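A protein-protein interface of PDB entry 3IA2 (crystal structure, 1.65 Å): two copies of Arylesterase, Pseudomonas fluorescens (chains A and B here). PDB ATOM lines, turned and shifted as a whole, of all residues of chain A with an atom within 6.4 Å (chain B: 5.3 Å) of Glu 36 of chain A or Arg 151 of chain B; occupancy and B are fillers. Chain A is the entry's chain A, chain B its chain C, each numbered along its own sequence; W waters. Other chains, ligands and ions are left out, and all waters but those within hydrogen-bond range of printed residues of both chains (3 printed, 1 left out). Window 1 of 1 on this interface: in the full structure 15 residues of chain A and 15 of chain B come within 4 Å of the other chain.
Of the 13 printed residues of chain A, 4 touch a printed residue of chain B.
Along chain A the printed residues that touch a printed residue of chain B span positions 16 to 178.
Hydrophobic or aromatic side chains of chain B within 4 Å of the printed part of chain A: Ala 152, Leu 184 and Leu 188.
Along chain B the printed residues that touch a printed residue of chain A span positions 147 to 188.
Among the printed residues, 11 pairs touch across the chains.
Among the printed residues, Asp or Glu carboxylates within 4 Å of a Lys or Arg side-chain nitrogen of the other chain: Glu 36 of chain A with Arg 151 of chain B (2.9 Å).
No position is printed for both chains.
Of the 11 pairs that touch across the chains among the printed residues, none has its exchanged pair printed and touching as well.
Printed residues of chain B within 4 Å of Glu 36 of chain A: Arg 151 (2.9 Å) and Leu 188 (3.5 Å).
Printed residues of chain A within 4 Å of Leu 188 of chain B: Glu 36 (3.5 Å) and Tyr 37 (3.6 Å).
Printed residues of chain A within 4 Å of Leu 184 of chain B: Gln 178.
Of the printed residues of chain B, Gln 178 of chain A touches Arg 151, Ala 152 and Leu 184.
Of the printed residues of chain B, Tyr 37 of chain A touches Leu 147, Lys 149, Asp 150, Arg 151 and Leu 188.
Of the printed residues of chain A, Ser 187 of chain B touches Trp 16 (3.5 Å).
Ala 186 of chain B touches none of the printed residues of chain A.
Gln 38 of chain A touches none of the printed residues of chain B.
Trp 16 of chain A touches Ser 187 of chain B (CZ2 to OG, 3.5 Å).
CD2 of Leu 188 of chain B touches O of Glu 36 of chain A, at 3.5 Å.
O of Leu 147 of chain B touches CE1 of Tyr 37 of chain A, 3.4 Å away.
O of Lys 149 of chain B touches CZ of Tyr 37 of chain A, 3.96 Å away.
Tyr 37 of chain A touches Asp 150 of chain B.
CD1 of Tyr 37 of chain A touches CD2 of Leu 188 of chain B, at 3.6 Å.
Ala 152 of chain B touches Gln 178 of chain A (CB to OE1, 3.8 Å).
CD of Gln 178 of chain A touches CD2 of Leu 184 of chain B, 3.9 Å away.
Water W3 lies within hydrogen-bond range of the backbone carbonyl oxygen of Leu 184 of chain B (2.7 Å), the side-chain carboxylate of Asp 33 of chain A (2.8 Å) and the side-chain amide nitrogen of Gln 178 of chain A (3.0 Å).
Water W1 lies within hydrogen-bond range of OE1 of Glu 36 of chain A, N of Leu 188 of chain B and NZ of Lys 14 of chain A.
Water W2 lies within hydrogen-bond range of the side-chain hydroxyl of Tyr 37 of chain A (2.8 Å), the side-chain carboxylate of Asp 150 of chain B (3.0 Å), the backbone NH of Ala 152 of chain B (3.2 Å) and the backbone NH of Arg 151 of chain B (3.4 Å).
NH1 of Arg 151 of chain B is in salt-bridge range of OE1 of Glu 36 of chain A.
The backbone NH (N) of Arg 151 of chain B is in hydrogen-bond range of the side-chain hydroxyl (OH) of Tyr 37 of chain A (2.9 Å).
NE2 of Gln 178 of chain A lies close to NH1 of Arg 151 of chain B.
The side-chain carboxylate (OD1) of Asp 150 of chain B sits close to the backbone NH (N) of Ala 152 of chain B, at 3.4 Å.
The side-chain carboxylate of Asp 150 of chain B is in hydrogen-bond range of the backbone NH of Gln 153 of chain B (3.0 Å).
O of Ala 183 of chain B lies within hydrogen-bond range of NH2 of Arg 151 of chain B (3.2 Å).
NH1 of Arg 151 of chain B is in hydrogen-bond range of O of Leu 184 of chain B.
NH1 of Arg 151 of chain B is in hydrogen-bond range of O of Ala 186 of chain B (3.1 Å).
The backbone carbonyl oxygen (O) of Ser 187 of chain B lies within hydrogen-bond range of the side-chain hydroxyl (OG1) of Thr 191 of chain B (2.8 Å).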
ATOM      1  N   LYS A  14     -36.391 -20.754 -19.810  1.00  0.00           N
ATOM      2  CA  LYS A  14     -36.748 -19.978 -20.986  1.00  0.00           C
ATOM      3  C   LYS A  14     -37.849 -20.711 -21.734  1.00  0.00           C
ATOM      4  O   LYS A  14     -37.828 -21.936 -21.842  1.00  0.00           O
ATOM      5  CB  LYS A  14     -35.547 -19.807 -21.913  1.00  0.00           C
ATOM      6  CG  LYS A  14     -34.304 -19.255 -21.246  1.00  0.00           C
ATOM      7  CD  LYS A  14     -33.216 -19.030 -22.286  1.00  0.00           C
ATOM      8  CE  LYS A  14     -31.857 -18.853 -21.641  1.00  0.00           C
ATOM      9  NZ  LYS A  14     -30.808 -18.623 -22.683  1.00  0.00           N
ATOM     10  N   TRP A  16     -39.546 -20.210 -25.399  1.00  0.00           N
ATOM     11  CA  TRP A  16     -39.462 -19.473 -26.661  1.00  0.00           C
ATOM     12  C   TRP A  16     -40.392 -20.018 -27.745  1.00  0.00           C
ATOM     13  O   TRP A  16     -40.535 -21.226 -27.902  1.00  0.00           O
ATOM     14  CB  TRP A  16     -38.036 -19.508 -27.220  1.00  0.00           C
ATOM     15  CG  TRP A  16     -37.017 -18.704 -26.468  1.00  0.00           C
ATOM     16  CD1 TRP A  16     -37.243 -17.826 -25.447  1.00  0.00           C
ATOM     17  CD2 TRP A  16     -35.607 -18.678 -26.717  1.00  0.00           C
ATOM     18  NE1 TRP A  16     -36.052 -17.270 -25.030  1.00  0.00           N
ATOM     19  CE2 TRP A  16     -35.034 -17.776 -25.796  1.00  0.00           C
ATOM     20  CE3 TRP A  16     -34.770 -19.336 -27.628  1.00  0.00           C
ATOM     21  CZ2 TRP A  16     -33.663 -17.518 -25.757  1.00  0.00           C
ATOM     22  CZ3 TRP A  16     -33.410 -19.078 -27.586  1.00  0.00           C
ATOM     23  CH2 TRP A  16     -32.870 -18.178 -26.657  1.00  0.00           C
ATOM     24  N   ALA A  32     -29.252 -23.831 -19.042  1.00  0.00           N
ATOM     25  CA  ALA A  32     -30.142 -23.756 -20.201  1.00  0.00           C
ATOM     26  C   ALA A  32     -29.462 -23.165 -21.438  1.00  0.00           C
ATOM     27  O   ALA A  32     -29.910 -23.393 -22.569  1.00  0.00           O
ATOM     28  CB  ALA A  32     -31.397 -22.971 -19.861  1.00  0.00           C
ATOM     29  N   ASP A  33     -28.385 -22.409 -21.229  1.00  0.00           N
ATOM     30  CA  ASP A  33     -27.696 -21.754 -22.342  1.00  0.00           C
ATOM     31  C   ASP A  33     -27.024 -22.741 -23.295  1.00  0.00           C
ATOM     32  O   ASP A  33     -26.781 -22.407 -24.452  1.00  0.00           O
ATOM     33  CB  ASP A  33     -26.672 -20.726 -21.847  1.00  0.00           C
ATOM     34  CG  ASP A  33     -27.319 -19.460 -21.307  1.00  0.00           C
ATOM     35  OD1 ASP A  33     -28.566 -19.416 -21.176  1.00  0.00           O
ATOM     36  OD2 ASP A  33     -26.576 -18.499 -21.016  1.00  0.00           O
ATOM     37  N   MET A  34     -26.730 -23.953 -22.823  1.00  0.00           N
ATOM     38  CA  MET A  34     -26.099 -24.947 -23.692  1.00  0.00           C
ATOM     39  C   MET A  34     -26.993 -25.278 -24.886  1.00  0.00           C
ATOM     40  O   MET A  34     -26.518 -25.785 -25.897  1.00  0.00           O
ATOM     41  CB  MET A  34     -25.730 -26.230 -22.930  1.00  0.00           C
ATOM     42  CG  MET A  34     -26.903 -27.150 -22.581  1.00  0.00           C
ATOM     43  SD  MET A  34     -26.407 -28.892 -22.410  1.00  0.00           S
ATOM     44  CE  MET A  34     -26.335 -29.393 -24.133  1.00  0.00           C
ATOM     45  N   TRP A  35     -28.284 -24.978 -24.764  1.00  0.00           N
ATOM     46  CA  TRP A  35     -29.263 -25.321 -25.800  1.00  0.00           C
ATOM     47  C   TRP A  35     -29.598 -24.160 -26.732  1.00  0.00           C
ATOM     48  O   TRP A  35     -30.442 -24.303 -27.624  1.00  0.00           O
ATOM     49  CB  TRP A  35     -30.572 -25.789 -25.158  1.00  0.00           C
ATOM     50  CG  TRP A  35     -30.458 -27.014 -24.316  1.00  0.00           C
ATOM     51  CD1 TRP A  35     -30.597 -27.091 -22.958  1.00  0.00           C
ATOM     52  CD2 TRP A  35     -30.193 -28.348 -24.771  1.00  0.00           C
ATOM     53  NE1 TRP A  35     -30.433 -28.391 -22.543  1.00  0.00           N
ATOM     54  CE2 TRP A  35     -30.185 -29.181 -23.635  1.00  0.00           C
ATOM     55  CE3 TRP A  35     -29.963 -28.918 -26.029  1.00  0.00           C
ATOM     56  CZ2 TRP A  35     -29.956 -30.556 -23.717  1.00  0.00           C
ATOM     57  CZ3 TRP A  35     -29.736 -30.285 -26.110  1.00  0.00           C
ATOM     58  CH2 TRP A  35     -29.737 -31.089 -24.962  1.00  0.00           C
ATOM     59  N   GLU A  36     -28.959 -23.011 -26.529  1.00  0.00           N
ATOM     60  CA  GLU A  36     -29.378 -21.796 -27.231  1.00  0.00           C
ATOM     61  C   GLU A  36     -29.504 -21.975 -28.746  1.00  0.00           C
ATOM     62  O   GLU A  36     -30.452 -21.482 -29.347  1.00  0.00           O
ATOM     63  CB  GLU A  36     -28.485 -20.596 -26.879  1.00  0.00           C
ATOM     64  CG  GLU A  36     -27.007 -20.785 -27.154  1.00  0.00           C
ATOM     65  CD  GLU A  36     -26.150 -19.754 -26.432  1.00  0.00           C
ATOM     66  OE1 GLU A  36     -26.716 -18.824 -25.825  1.00  0.00           O
ATOM     67  OE2 GLU A  36     -24.909 -19.880 -26.466  1.00  0.00           O
ATOM     68  N   TYR A  37     -28.557 -22.680 -29.357  1.00  0.00           N
ATOM     69  CA  TYR A  37     -28.574 -22.852 -30.811  1.00  0.00           C
ATOM     70  C   TYR A  37     -29.686 -23.792 -31.282  1.00  0.00           C
ATOM     71  O   TYR A  37     -30.338 -23.532 -32.296  1.00  0.00           O
ATOM     72  CB  TYR A  37     -27.210 -23.321 -31.324  1.00  0.00           C
ATOM     73  CG  TYR A  37     -26.098 -22.334 -31.047  1.00  0.00           C
ATOM     74  CD1 TYR A  37     -25.832 -21.291 -31.926  1.00  0.00           C
ATOM     75  CD2 TYR A  37     -25.320 -22.440 -29.900  1.00  0.00           C
ATOM     76  CE1 TYR A  37     -24.820 -20.378 -31.670  1.00  0.00           C
ATOM     77  CE2 TYR A  37     -24.303 -21.533 -29.637  1.00  0.00           C
ATOM     78  CZ  TYR A  37     -24.059 -20.507 -30.526  1.00  0.00           C
ATOM     79  OH  TYR A  37     -23.050 -19.606 -30.265  1.00  0.00           O
ATOM     80  N   GLN A  38     -29.907 -24.882 -30.549  1.00  0.00           N
ATOM     81  CA  GLN A  38     -31.009 -25.789 -30.882  1.00  0.00           C
ATOM     82  C   GLN A  38     -32.361 -25.103 -30.710  1.00  0.00           C
ATOM     83  O   GLN A  38     -33.271 -25.297 -31.519  1.00  0.00           O
ATOM     84  CB  GLN A  38     -30.956 -27.071 -30.043  1.00  0.00           C
ATOM     85  CG  GLN A  38     -29.873 -28.041 -30.476  1.00  0.00           C
ATOM     86  CD  GLN A  38     -28.489 -27.544 -30.125  1.00  0.00           C
ATOM     87  OE1 GLN A  38     -28.204 -27.253 -28.962  1.00  0.00           O
ATOM     88  NE2 GLN A  38     -27.618 -27.448 -31.124  1.00  0.00           N
ATOM     89  N   MET A  39     -32.486 -24.296 -29.659  1.00  0.00           N
ATOM     90  CA  MET A  39     -33.726 -23.569 -29.406  1.00  0.00           C
ATOM     91  C   MET A  39     -34.032 -22.556 -30.511  1.00  0.00           C
ATOM     92  O   MET A  39     -35.160 -22.479 -30.997  1.00  0.00           O
ATOM     93  CB  MET A  39     -33.687 -22.886 -28.032  1.00  0.00           C
ATOM     94  CG  MET A  39     -33.649 -23.870 -26.867  1.00  0.00           C
ATOM     95  SD  MET A  39     -33.618 -23.069 -25.249  1.00  0.00           S
ATOM     96  CE  MET A  39     -35.285 -22.430 -25.128  1.00  0.00           C
ATOM     97  N   GLU A  40     -33.030 -21.777 -30.909  1.00  0.00           N
ATOM     98  CA  GLU A  40     -33.223 -20.798 -31.974  1.00  0.00           C
ATOM     99  C   GLU A  40     -33.540 -21.501 -33.291  1.00  0.00           C
ATOM    100  O   GLU A  40     -34.387 -21.050 -34.060  1.00  0.00           O
ATOM    101  CB  GLU A  40     -31.985 -19.908 -32.132  1.00  0.00           C
ATOM    102  CG  GLU A  40     -32.177 -18.721 -33.077  1.00  0.00           C
ATOM    103  CD  GLU A  40     -32.080 -19.101 -34.550  1.00  0.00           C
ATOM    104  OE1 GLU A  40     -31.436 -20.121 -34.871  1.00  0.00           O
ATOM    105  OE2 GLU A  40     -32.642 -18.367 -35.388  1.00  0.00           O
ATOM    106  N   TYR A  41     -32.854 -22.610 -33.543  1.00  0.00           N
ATOM    107  CA  TYR A  41     -33.053 -23.368 -34.774  1.00  0.00           C
ATOM    108  C   TYR A  41     -34.489 -23.869 -34.897  1.00  0.00           C
ATOM    109  O   TYR A  41     -35.130 -23.701 -35.936  1.00  0.00           O
ATOM    110  CB  TYR A  41     -32.086 -24.547 -34.837  1.00  0.00           C
ATOM    111  CG  TYR A  41     -32.167 -25.345 -36.121  1.00  0.00           C
ATOM    112  CD1 TYR A  41     -31.368 -25.022 -37.211  1.00  0.00           C
ATOM    113  CD2 TYR A  41     -33.046 -26.415 -36.246  1.00  0.00           C
ATOM    114  CE1 TYR A  41     -31.437 -25.743 -38.392  1.00  0.00           C
ATOM    115  CE2 TYR A  41     -33.120 -27.149 -37.424  1.00  0.00           C
ATOM    116  CZ  TYR A  41     -32.314 -26.805 -38.492  1.00  0.00           C
ATOM    117  OH  TYR A  41     -32.377 -27.525 -39.666  1.00  0.00           O
ATOM    118  N   GLN A 178     -17.014 -19.466 -22.183  1.00  0.00           N
ATOM    119  CA  GLN A 178     -18.441 -19.454 -21.837  1.00  0.00           C
ATOM    120  C   GLN A 178     -18.801 -20.672 -20.987  1.00  0.00           C
ATOM    121  O   GLN A 178     -19.602 -20.578 -20.051  1.00  0.00           O
ATOM    122  CB  GLN A 178     -19.315 -19.416 -23.096  1.00  0.00           C
ATOM    123  CG  GLN A 178     -20.815 -19.418 -22.799  1.00  0.00           C
ATOM    124  CD  GLN A 178     -21.671 -19.308 -24.049  1.00  0.00           C
ATOM    125  OE1 GLN A 178     -21.223 -19.615 -25.153  1.00  0.00           O
ATOM    126  NE2 GLN A 178     -22.912 -18.874 -23.877  1.00  0.00           N
ATOM    127  N   GLU B 146     -22.160 -15.874 -38.506  1.00  0.00           N
ATOM    128  CA  GLU B 146     -21.101 -16.179 -37.550  1.00  0.00           C
ATOM    129  C   GLU B 146     -21.640 -16.322 -36.122  1.00  0.00           C
ATOM    130  O   GLU B 146     -21.199 -17.192 -35.373  1.00  0.00           O
ATOM    131  CB  GLU B 146     -19.985 -15.131 -37.617  1.00  0.00           C
ATOM    132  CG  GLU B 146     -19.262 -15.097 -38.962  1.00  0.00           C
ATOM    133  CD  GLU B 146     -18.787 -16.476 -39.398  1.00  0.00           C
ATOM    134  OE1 GLU B 146     -18.056 -17.123 -38.620  1.00  0.00           O
ATOM    135  OE2 GLU B 146     -19.145 -16.919 -40.515  1.00  0.00           O
ATOM    136  N   LEU B 147     -22.602 -15.477 -35.754  1.00  0.00           N
ATOM    137  CA  LEU B 147     -23.224 -15.556 -34.428  1.00  0.00           C
ATOM    138  C   LEU B 147     -23.964 -16.878 -34.213  1.00  0.00           C
ATOM    139  O   LEU B 147     -23.957 -17.432 -33.113  1.00  0.00           O
ATOM    140  CB  LEU B 147     -24.187 -14.387 -34.215  1.00  0.00           C
ATOM    141  CG  LEU B 147     -23.589 -12.999 -33.987  1.00  0.00           C
ATOM    142  CD1 LEU B 147     -24.643 -11.920 -34.203  1.00  0.00           C
ATOM    143  CD2 LEU B 147     -22.988 -12.895 -32.589  1.00  0.00           C
ATOM    144  N   LYS B 149     -23.180 -19.630 -35.372  1.00  0.00           N
ATOM    145  CA  LYS B 149     -22.199 -20.707 -35.280  1.00  0.00           C
ATOM    146  C   LYS B 149     -21.495 -20.683 -33.928  1.00  0.00           C
ATOM    147  O   LYS B 149     -21.427 -21.697 -33.234  1.00  0.00           O
ATOM    148  CB  LYS B 149     -21.156 -20.586 -36.390  1.00  0.00           C
ATOM    149  CG  LYS B 149     -21.670 -20.919 -37.777  1.00  0.00           C
ATOM    150  CD  LYS B 149     -20.580 -20.703 -38.813  1.00  0.00           C
ATOM    151  CE  LYS B 149     -21.059 -21.074 -40.203  1.00  0.00           C
ATOM    152  NZ  LYS B 149     -19.984 -20.853 -41.212  1.00  0.00           N
ATOM    153  N   ASP B 150     -20.970 -19.517 -33.561  1.00  0.00           N
ATOM    154  CA  ASP B 150     -20.171 -19.385 -32.350  1.00  0.00           C
ATOM    155  C   ASP B 150     -20.196 -17.935 -31.879  1.00  0.00           C
ATOM    156  O   ASP B 150     -19.294 -17.162 -32.192  1.00  0.00           O
ATOM    157  CB  ASP B 150     -18.732 -19.831 -32.639  1.00  0.00           C
ATOM    158  CG  ASP B 150     -17.856 -19.868 -31.396  1.00  0.00           C
ATOM    159  OD1 ASP B 150     -18.273 -19.350 -30.338  1.00  0.00           O
ATOM    160  OD2 ASP B 150     -16.734 -20.413 -31.489  1.00  0.00           O
ATOM    161  N   ARG B 151     -21.230 -17.560 -31.135  1.00  0.00           N
ATOM    162  CA  ARG B 151     -21.364 -16.167 -30.717  1.00  0.00           C
ATOM    163  C   ARG B 151     -20.306 -15.766 -29.688  1.00  0.00           C
ATOM    164  O   ARG B 151     -19.898 -14.610 -29.631  1.00  0.00           O
ATOM    165  CB  ARG B 151     -22.776 -15.869 -30.200  1.00  0.00           C
ATOM    166  CG  ARG B 151     -23.014 -16.233 -28.758  1.00  0.00           C
ATOM    167  CD  ARG B 151     -24.340 -15.664 -28.262  1.00  0.00           C
ATOM    168  NE  ARG B 151     -24.780 -16.347 -27.053  1.00  0.00           N
ATOM    169  CZ  ARG B 151     -24.825 -15.791 -25.847  1.00  0.00           C
ATOM    170  NH1 ARG B 151     -25.237 -16.508 -24.811  1.00  0.00           N
ATOM    171  NH2 ARG B 151     -24.476 -14.523 -25.679  1.00  0.00           N
ATOM    172  N   ALA B 152     -19.854 -16.724 -28.887  1.00  0.00           N
ATOM    173  CA  ALA B 152     -18.839 -16.437 -27.881  1.00  0.00           C
ATOM    174  C   ALA B 152     -17.541 -15.958 -28.527  1.00  0.00           C
ATOM    175  O   ALA B 152     -16.968 -14.956 -28.106  1.00  0.00           O
ATOM    176  CB  ALA B 152     -18.590 -17.657 -26.993  1.00  0.00           C
ATOM    177  N   GLN B 153     -17.084 -16.661 -29.560  1.00  0.00           N
ATOM    178  CA  GLN B 153     -15.860 -16.251 -30.250  1.00  0.00           C
ATOM    179  C   GLN B 153     -16.083 -14.995 -31.091  1.00  0.00           C
ATOM    180  O   GLN B 153     -15.170 -14.181 -31.255  1.00  0.00           O
ATOM    181  CB  GLN B 153     -15.288 -17.378 -31.108  1.00  0.00           C
ATOM    182  CG  GLN B 153     -13.895 -17.073 -31.650  1.00  0.00           C
ATOM    183  CD  GLN B 153     -12.878 -16.836 -30.547  1.00  0.00           C
ATOM    184  OE1 GLN B 153     -12.910 -17.489 -29.506  1.00  0.00           O
ATOM    185  NE2 GLN B 153     -11.968 -15.894 -30.772  1.00  0.00           N
ATOM    186  N   PHE B 154     -17.294 -14.827 -31.613  1.00  0.00           N
ATOM    187  CA  PHE B 154     -17.628 -13.596 -32.324  1.00  0.00           C
ATOM    188  C   PHE B 154     -17.424 -12.388 -31.410  1.00  0.00           C
ATOM    189  O   PHE B 154     -16.781 -11.412 -31.790  1.00  0.00           O
ATOM    190  CB  PHE B 154     -19.068 -13.616 -32.848  1.00  0.00           C
ATOM    191  CG  PHE B 154     -19.442 -12.374 -33.619  1.00  0.00           C
ATOM    192  CD1 PHE B 154     -19.332 -12.338 -35.002  1.00  0.00           C
ATOM    193  CD2 PHE B 154     -19.883 -11.239 -32.957  1.00  0.00           C
ATOM    194  CE1 PHE B 154     -19.662 -11.191 -35.709  1.00  0.00           C
ATOM    195  CE2 PHE B 154     -20.219 -10.088 -33.659  1.00  0.00           C
ATOM    196  CZ  PHE B 154     -20.110 -10.066 -35.036  1.00  0.00           C
ATOM    197  N   ILE B 155     -17.982 -12.458 -30.206  1.00  0.00           N
ATOM    198  CA  ILE B 155     -17.844 -11.376 -29.235  1.00  0.00           C
ATOM    199  C   ILE B 155     -16.376 -11.106 -28.922  1.00  0.00           C
ATOM    200  O   ILE B 155     -15.940  -9.953 -28.880  1.00  0.00           O
ATOM    201  CB  ILE B 155     -18.587 -11.696 -27.919  1.00  0.00           C
ATOM    202  CG1 ILE B 155     -20.089 -11.854 -28.174  1.00  0.00           C
ATOM    203  CG2 ILE B 155     -18.325 -10.608 -26.879  1.00  0.00           C
ATOM    204  CD1 ILE B 155     -20.802 -12.664 -27.106  1.00  0.00           C
ATOM    205  N   SER B 156     -15.617 -12.175 -28.692  1.00  0.00           N
ATOM    206  CA  SER B 156     -14.206 -12.048 -28.357  1.00  0.00           C
ATOM    207  C   SER B 156     -13.446 -11.345 -29.477  1.00  0.00           C
ATOM    208  O   SER B 156     -12.641 -10.447 -29.223  1.00  0.00           O
ATOM    209  CB  SER B 156     -13.595 -13.425 -28.086  1.00  0.00           C
ATOM    210  OG  SER B 156     -12.280 -13.315 -27.569  1.00  0.00           O
ATOM    211  N   ALA B 183     -21.461  -9.743 -22.283  1.00  0.00           N
ATOM    212  CA  ALA B 183     -22.072 -10.127 -23.550  1.00  0.00           C
ATOM    213  C   ALA B 183     -22.629 -11.554 -23.511  1.00  0.00           C
ATOM    214  O   ALA B 183     -23.668 -11.847 -24.108  1.00  0.00           O
ATOM    215  CB  ALA B 183     -21.055  -9.979 -24.677  1.00  0.00           C
ATOM    216  N   LEU B 184     -21.939 -12.442 -22.801  1.00  0.00           N
ATOM    217  CA  LEU B 184     -22.354 -13.839 -22.723  1.00  0.00           C
ATOM    218  C   LEU B 184     -23.638 -14.023 -21.913  1.00  0.00           C
ATOM    219  O   LEU B 184     -24.315 -15.041 -22.040  1.00  0.00           O
ATOM    220  CB  LEU B 184     -21.228 -14.704 -22.155  1.00  0.00           C
ATOM    221  CG  LEU B 184     -20.040 -14.882 -23.102  1.00  0.00           C
ATOM    222  CD1 LEU B 184     -18.899 -15.589 -22.381  1.00  0.00           C
ATOM    223  CD2 LEU B 184     -20.464 -15.656 -24.345  1.00  0.00           C
ATOM    224  N   LEU B 185     -23.965 -13.039 -21.079  1.00  0.00           N
ATOM    225  CA  LEU B 185     -25.204 -13.080 -20.311  1.00  0.00           C
ATOM    226  C   LEU B 185     -26.416 -13.023 -21.234  1.00  0.00           C
ATOM    227  O   LEU B 185     -27.479 -13.564 -20.918  1.00  0.00           O
ATOM    228  CB  LEU B 185     -25.274 -11.896 -19.342  1.00  0.00           C
ATOM    229  CG  LEU B 185     -24.222 -11.775 -18.236  1.00  0.00           C
ATOM    230  CD1 LEU B 185     -24.474 -10.517 -17.417  1.00  0.00           C
ATOM    231  CD2 LEU B 185     -24.229 -13.010 -17.347  1.00  0.00           C
ATOM    232  N   ALA B 186     -26.245 -12.358 -22.370  1.00  0.00           N
ATOM    233  CA  ALA B 186     -27.347 -12.078 -23.289  1.00  0.00           C
ATOM    234  C   ALA B 186     -27.917 -13.313 -23.985  1.00  0.00           C
ATOM    235  O   ALA B 186     -27.290 -14.373 -24.034  1.00  0.00           O
ATOM    236  CB  ALA B 186     -26.912 -11.045 -24.326  1.00  0.00           C
ATOM    237  N   SER B 187     -29.121 -13.150 -24.525  1.00  0.00           N
ATOM    238  CA  SER B 187     -29.786 -14.186 -25.302  1.00  0.00           C
ATOM    239  C   SER B 187     -29.214 -14.284 -26.712  1.00  0.00           C
ATOM    240  O   SER B 187     -28.990 -13.265 -27.367  1.00  0.00           O
ATOM    241  CB  SER B 187     -31.272 -13.851 -25.414  1.00  0.00           C
ATOM    242  OG  SER B 187     -31.881 -14.588 -26.458  1.00  0.00           O
ATOM    243  N   LEU B 188     -29.000 -15.508 -27.190  1.00  0.00           N
ATOM    244  CA  LEU B 188     -28.597 -15.710 -28.581  1.00  0.00           C
ATOM    245  C   LEU B 188     -29.631 -15.103 -29.535  1.00  0.00           C
ATOM    246  O   LEU B 188     -29.277 -14.432 -30.505  1.00  0.00           O
ATOM    247  CB  LEU B 188     -28.417 -17.198 -28.892  1.00  0.00           C
ATOM    248  CG  LEU B 188     -28.229 -17.529 -30.377  1.00  0.00           C
ATOM    249  CD1 LEU B 188     -26.933 -16.928 -30.908  1.00  0.00           C
ATOM    250  CD2 LEU B 188     -28.253 -19.031 -30.606  1.00  0.00           C
ATOM    251  N   THR B 191     -29.568 -11.307 -29.435  1.00  0.00           N
ATOM    252  CA  THR B 191     -28.339 -10.841 -30.064  1.00  0.00           C
ATOM    253  C   THR B 191     -28.485 -10.791 -31.586  1.00  0.00           C
ATOM    254  O   THR B 191     -28.091  -9.813 -32.229  1.00  0.00           O
ATOM    255  CB  THR B 191     -27.136 -11.725 -29.662  1.00  0.00           C
ATOM    256  OG1 THR B 191     -26.928 -11.623 -28.246  1.00  0.00           O
ATOM    257  CG2 THR B 191     -25.867 -11.276 -30.383  1.00  0.00           C
HETATM  258  O   HOH W   1     -28.988 -17.595 -25.026  1.00  0.00           O
HETATM  259  O   HOH W   2     -20.700 -19.794 -28.664  1.00  0.00           O
HETATM  260  O   HOH W   3     -23.968 -17.618 -21.318  1.00  0.00           O
